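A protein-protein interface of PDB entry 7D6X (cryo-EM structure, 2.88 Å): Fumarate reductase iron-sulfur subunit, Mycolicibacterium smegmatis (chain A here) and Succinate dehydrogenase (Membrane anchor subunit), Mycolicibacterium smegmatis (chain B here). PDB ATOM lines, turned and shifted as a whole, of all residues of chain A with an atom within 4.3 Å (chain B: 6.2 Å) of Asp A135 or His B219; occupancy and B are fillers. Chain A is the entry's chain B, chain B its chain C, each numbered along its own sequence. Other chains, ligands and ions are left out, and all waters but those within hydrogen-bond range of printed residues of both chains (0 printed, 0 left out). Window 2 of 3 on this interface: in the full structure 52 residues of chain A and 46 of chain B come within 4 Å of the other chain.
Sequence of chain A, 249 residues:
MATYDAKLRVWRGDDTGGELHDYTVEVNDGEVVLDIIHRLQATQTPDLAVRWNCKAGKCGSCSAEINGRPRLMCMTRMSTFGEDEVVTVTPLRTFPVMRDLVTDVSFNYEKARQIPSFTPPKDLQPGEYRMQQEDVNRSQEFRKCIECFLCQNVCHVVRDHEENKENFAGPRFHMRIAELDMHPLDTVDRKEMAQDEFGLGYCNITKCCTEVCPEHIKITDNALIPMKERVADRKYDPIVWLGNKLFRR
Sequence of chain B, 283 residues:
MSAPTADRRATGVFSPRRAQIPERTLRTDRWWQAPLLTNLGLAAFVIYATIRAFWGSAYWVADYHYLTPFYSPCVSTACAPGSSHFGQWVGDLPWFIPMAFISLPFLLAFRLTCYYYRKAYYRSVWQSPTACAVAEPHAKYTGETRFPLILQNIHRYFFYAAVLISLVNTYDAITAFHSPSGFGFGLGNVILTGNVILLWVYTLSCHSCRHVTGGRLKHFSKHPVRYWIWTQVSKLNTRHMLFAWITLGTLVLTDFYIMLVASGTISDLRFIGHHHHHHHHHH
The side-chain carboxylate (OD1) of Asp A135 lies within hydrogen-bond range of the backbone NH (N) of Phe B220 (3.5 Å). OD1 of Asp A135 sits at hydrogen-bond distance from N of Ser B221 (3.1 Å).
O of His B219 sits at hydrogen-bond distance from ND1 of His B223, at 3.0 Å.
CB of Ser B221 touches CG of Gln A132, 3.8 Å away. O of Glu A134 touches CD2 of Phe B220, 3.8 Å away. Ser B221 touches Glu A134 (CB to OE2, 3.5 Å). OD2 of Asp A135 touches ND1 of His B219, 3.8 Å away. O of Pro A184 touches CE1 of His B219, 3.1 Å away.
Asp A135 touches three residues of chain B. His B219 touches just these residues of chain A: Asp A135 and Pro A184. Printed residues of chain B within 4 Å of Pro A184: His B219 (3.1 Å). Printed residues of chain B within 4 Å of Glu A134: Phe B220 (3.8 Å) and Ser B221 (3.5 Å). Printed residues of chain B within 4 Å of Gln A132: Ser B221 (3.8 Å). Of the printed residues of chain A, Ser B221 touches Gln A132 (3.8 Å), Glu A134 (3.5 Å) and Asp A135 (3.1 Å). Printed residues of chain A within 4 Å of Phe B220: Glu A134 and Asp A135. His B223 touches none of the printed residues of chain A. Val A136 touches none of the printed residues of chain B.
Of the 8 printed residues of chain A, 4 touch a printed residue of chain B. Of the 7 printed residues of chain B, 3 touch a printed residue of chain A. Among the printed residues, no Asp or Glu carboxylate lies within 4 Å of a Lys or Arg side-chain nitrogen of the other chain.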
ATOM      1  N   GLN A 132     -15.700 -21.944  24.156  1.00  0.00           N
ATOM      2  CA  GLN A 132     -15.137 -20.662  23.772  1.00  0.00           C
ATOM      3  C   GLN A 132     -13.651 -20.811  23.478  1.00  0.00           C
ATOM      4  O   GLN A 132     -12.996 -21.749  23.929  1.00  0.00           O
ATOM      5  CB  GLN A 132     -15.361 -19.623  24.864  1.00  0.00           C
ATOM      6  CG  GLN A 132     -16.812 -19.441  25.233  1.00  0.00           C
ATOM      7  CD  GLN A 132     -17.642 -18.936  24.081  1.00  0.00           C
ATOM      8  OE1 GLN A 132     -17.208 -18.078  23.319  1.00  0.00           O
ATOM      9  NE2 GLN A 132     -18.848 -19.466  23.946  1.00  0.00           N
ATOM     10  N   GLN A 133     -13.123 -19.865  22.704  1.00  0.00           N
ATOM     11  CA  GLN A 133     -11.750 -19.983  22.226  1.00  0.00           C
ATOM     12  C   GLN A 133     -10.748 -19.915  23.371  1.00  0.00           C
ATOM     13  O   GLN A 133      -9.730 -20.617  23.358  1.00  0.00           O
ATOM     14  CB  GLN A 133     -11.468 -18.900  21.192  1.00  0.00           C
ATOM     15  CG  GLN A 133     -10.076 -18.947  20.610  1.00  0.00           C
ATOM     16  CD  GLN A 133      -9.883 -20.088  19.643  1.00  0.00           C
ATOM     17  OE1 GLN A 133      -9.243 -21.085  19.961  1.00  0.00           O
ATOM     18  NE2 GLN A 133     -10.428 -19.942  18.446  1.00  0.00           N
ATOM     19  N   GLU A 134     -11.015 -19.078  24.374  1.00  0.00           N
ATOM     20  CA  GLU A 134     -10.105 -18.991  25.510  1.00  0.00           C
ATOM     21  C   GLU A 134     -10.115 -20.253  26.355  1.00  0.00           C
ATOM     22  O   GLU A 134      -9.160 -20.489  27.101  1.00  0.00           O
ATOM     23  CB  GLU A 134     -10.445 -17.783  26.378  1.00  0.00           C
ATOM     24  CG  GLU A 134     -11.869 -17.738  26.865  1.00  0.00           C
ATOM     25  CD  GLU A 134     -12.752 -16.902  25.974  1.00  0.00           C
ATOM     26  OE1 GLU A 134     -12.374 -16.671  24.809  1.00  0.00           O
ATOM     27  OE2 GLU A 134     -13.826 -16.470  26.435  1.00  0.00           O
ATOM     28  N   ASP A 135     -11.164 -21.070  26.255  1.00  0.00           N
ATOM     29  CA  ASP A 135     -11.190 -22.337  26.974  1.00  0.00           C
ATOM     30  C   ASP A 135     -10.363 -23.400  26.265  1.00  0.00           C
ATOM     31  O   ASP A 135      -9.735 -24.239  26.918  1.00  0.00           O
ATOM     32  CB  ASP A 135     -12.628 -22.814  27.145  1.00  0.00           C
ATOM     33  CG  ASP A 135     -13.475 -21.833  27.909  1.00  0.00           C
ATOM     34  OD1 ASP A 135     -12.978 -20.730  28.193  1.00  0.00           O
ATOM     35  OD2 ASP A 135     -14.636 -22.159  28.225  1.00  0.00           O
ATOM     36  N   VAL A 136     -10.346 -23.382  24.932  1.00  0.00           N
ATOM     37  CA  VAL A 136      -9.603 -24.379  24.171  1.00  0.00           C
ATOM     38  C   VAL A 136      -8.170 -23.961  23.892  1.00  0.00           C
ATOM     39  O   VAL A 136      -7.387 -24.781  23.390  1.00  0.00           O
ATOM     40  CB  VAL A 136     -10.306 -24.684  22.834  1.00  0.00           C
ATOM     41  CG1 VAL A 136     -11.767 -24.981  23.066  1.00  0.00           C
ATOM     42  CG2 VAL A 136     -10.152 -23.528  21.882  1.00  0.00           C
ATOM     43  N   ASN A 137      -7.806 -22.710  24.186  1.00  0.00           N
ATOM     44  CA  ASN A 137      -6.469 -22.227  23.860  1.00  0.00           C
ATOM     45  C   ASN A 137      -5.387 -23.011  24.588  1.00  0.00           C
ATOM     46  O   ASN A 137      -4.319 -23.271  24.025  1.00  0.00           O
ATOM     47  CB  ASN A 137      -6.356 -20.744  24.197  1.00  0.00           C
ATOM     48  CG  ASN A 137      -6.651 -19.859  23.017  1.00  0.00           C
ATOM     49  OD1 ASN A 137      -6.560 -20.286  21.871  1.00  0.00           O
ATOM     50  ND2 ASN A 137      -6.998 -18.612  23.288  1.00  0.00           N
ATOM     51  N   MET A 182      -7.162 -30.013  31.143  1.00  0.00           N
ATOM     52  CA  MET A 182      -7.551 -28.656  30.798  1.00  0.00           C
ATOM     53  C   MET A 182      -8.632 -28.601  29.731  1.00  0.00           C
ATOM     54  O   MET A 182      -9.061 -27.504  29.365  1.00  0.00           O
ATOM     55  CB  MET A 182      -6.328 -27.863  30.336  1.00  0.00           C
ATOM     56  CG  MET A 182      -5.244 -27.760  31.382  1.00  0.00           C
ATOM     57  SD  MET A 182      -3.734 -27.014  30.761  1.00  0.00           S
ATOM     58  CE  MET A 182      -2.678 -27.172  32.195  1.00  0.00           C
ATOM     59  N   PRO A 184     -12.129 -28.279  28.325  1.00  0.00           N
ATOM     60  CA  PRO A 184     -13.302 -27.702  28.997  1.00  0.00           C
ATOM     61  C   PRO A 184     -14.482 -28.645  29.122  1.00  0.00           C
ATOM     62  O   PRO A 184     -15.410 -28.342  29.879  1.00  0.00           O
ATOM     63  CB  PRO A 184     -13.646 -26.496  28.116  1.00  0.00           C
ATOM     64  CG  PRO A 184     -13.056 -26.810  26.799  1.00  0.00           C
ATOM     65  CD  PRO A 184     -11.811 -27.576  27.073  1.00  0.00           C
ATOM     66  N   LEU B 217      -8.268 -22.857  37.053  1.00  0.00           N
ATOM     67  CA  LEU B 217      -9.632 -22.858  36.561  1.00  0.00           C
ATOM     68  C   LEU B 217      -9.738 -23.708  35.306  1.00  0.00           C
ATOM     69  O   LEU B 217      -8.779 -23.845  34.543  1.00  0.00           O
ATOM     70  CB  LEU B 217     -10.104 -21.436  36.264  1.00  0.00           C
ATOM     71  CG  LEU B 217     -10.010 -20.417  37.391  1.00  0.00           C
ATOM     72  CD1 LEU B 217     -10.298 -19.046  36.842  1.00  0.00           C
ATOM     73  CD2 LEU B 217     -10.972 -20.755  38.500  1.00  0.00           C
ATOM     74  N   LYS B 218     -10.918 -24.282  35.097  1.00  0.00           N
ATOM     75  CA  LYS B 218     -11.205 -25.018  33.875  1.00  0.00           C
ATOM     76  C   LYS B 218     -11.887 -24.156  32.826  1.00  0.00           C
ATOM     77  O   LYS B 218     -11.578 -24.274  31.637  1.00  0.00           O
ATOM     78  CB  LYS B 218     -12.073 -26.242  34.182  1.00  0.00           C
ATOM     79  CG  LYS B 218     -12.522 -27.002  32.948  1.00  0.00           C
ATOM     80  CD  LYS B 218     -12.992 -28.403  33.284  1.00  0.00           C
ATOM     81  CE  LYS B 218     -11.848 -29.395  33.230  1.00  0.00           C
ATOM     82  NZ  LYS B 218     -12.285 -30.719  32.718  1.00  0.00           N
ATOM     83  N   HIS B 219     -12.795 -23.279  33.238  1.00  0.00           N
ATOM     84  CA  HIS B 219     -13.509 -22.390  32.331  1.00  0.00           C
ATOM     85  C   HIS B 219     -13.016 -20.970  32.555  1.00  0.00           C
ATOM     86  O   HIS B 219     -13.295 -20.369  33.596  1.00  0.00           O
ATOM     87  CB  HIS B 219     -15.016 -22.482  32.548  1.00  0.00           C
ATOM     88  CG  HIS B 219     -15.576 -23.846  32.308  1.00  0.00           C
ATOM     89  ND1 HIS B 219     -15.636 -24.414  31.055  1.00  0.00           N
ATOM     90  CD2 HIS B 219     -16.101 -24.757  33.159  1.00  0.00           C
ATOM     91  CE1 HIS B 219     -16.175 -25.617  31.145  1.00  0.00           C
ATOM     92  NE2 HIS B 219     -16.466 -25.849  32.411  1.00  0.00           N
ATOM     93  N   PHE B 220     -12.277 -20.440  31.583  1.00  0.00           N
ATOM     94  CA  PHE B 220     -11.854 -19.049  31.640  1.00  0.00           C
ATOM     95  C   PHE B 220     -12.964 -18.104  31.209  1.00  0.00           C
ATOM     96  O   PHE B 220     -13.052 -16.985  31.722  1.00  0.00           O
ATOM     97  CB  PHE B 220     -10.623 -18.841  30.763  1.00  0.00           C
ATOM     98  CG  PHE B 220      -9.340 -19.221  31.428  1.00  0.00           C
ATOM     99  CD1 PHE B 220      -9.130 -18.935  32.761  1.00  0.00           C
ATOM    100  CD2 PHE B 220      -8.343 -19.863  30.725  1.00  0.00           C
ATOM    101  CE1 PHE B 220      -7.956 -19.282  33.376  1.00  0.00           C
ATOM    102  CE2 PHE B 220      -7.166 -20.212  31.340  1.00  0.00           C
ATOM    103  CZ  PHE B 220      -6.976 -19.923  32.667  1.00  0.00           C
ATOM    104  N   SER B 221     -13.817 -18.534  30.281  1.00  0.00           N
ATOM    105  CA  SER B 221     -14.918 -17.702  29.814  1.00  0.00           C
ATOM    106  C   SER B 221     -15.898 -17.364  30.925  1.00  0.00           C
ATOM    107  O   SER B 221     -16.645 -16.387  30.806  1.00  0.00           O
ATOM    108  CB  SER B 221     -15.649 -18.414  28.680  1.00  0.00           C
ATOM    109  OG  SER B 221     -16.259 -19.604  29.151  1.00  0.00           O
ATOM    110  N   LYS B 222     -15.918 -18.153  31.992  1.00  0.00           N
ATOM    111  CA  LYS B 222     -16.801 -17.912  33.121  1.00  0.00           C
ATOM    112  C   LYS B 222     -16.186 -16.977  34.153  1.00  0.00           C
ATOM    113  O   LYS B 222     -16.872 -16.588  35.101  1.00  0.00           O
ATOM    114  CB  LYS B 222     -17.164 -19.251  33.764  1.00  0.00           C
ATOM    115  CG  LYS B 222     -18.521 -19.288  34.424  1.00  0.00           C
ATOM    116  CD  LYS B 222     -18.769 -20.643  35.067  1.00  0.00           C
ATOM    117  CE  LYS B 222     -19.733 -20.535  36.240  1.00  0.00           C
ATOM    118  NZ  LYS B 222     -19.146 -19.794  37.384  1.00  0.00           N
ATOM    119  N   HIS B 223     -14.917 -16.608  33.986  1.00  0.00           N
ATOM    120  CA  HIS B 223     -14.194 -15.759  34.930  1.00  0.00           C
ATOM    121  C   HIS B 223     -13.428 -14.709  34.141  1.00  0.00           C
ATOM    122  O   HIS B 223     -12.326 -14.968  33.645  1.00  0.00           O
ATOM    123  CB  HIS B 223     -13.258 -16.587  35.804  1.00  0.00           C
ATOM    124  CG  HIS B 223     -13.956 -17.647  36.594  1.00  0.00           C
ATOM    125  ND1 HIS B 223     -13.990 -18.965  36.202  1.00  0.00           N
ATOM    126  CD2 HIS B 223     -14.658 -17.581  37.749  1.00  0.00           C
ATOM    127  CE1 HIS B 223     -14.676 -19.667  37.083  1.00  0.00           C
ATOM    128  NE2 HIS B 223     -15.092 -18.850  38.032  1.00  0.00           N
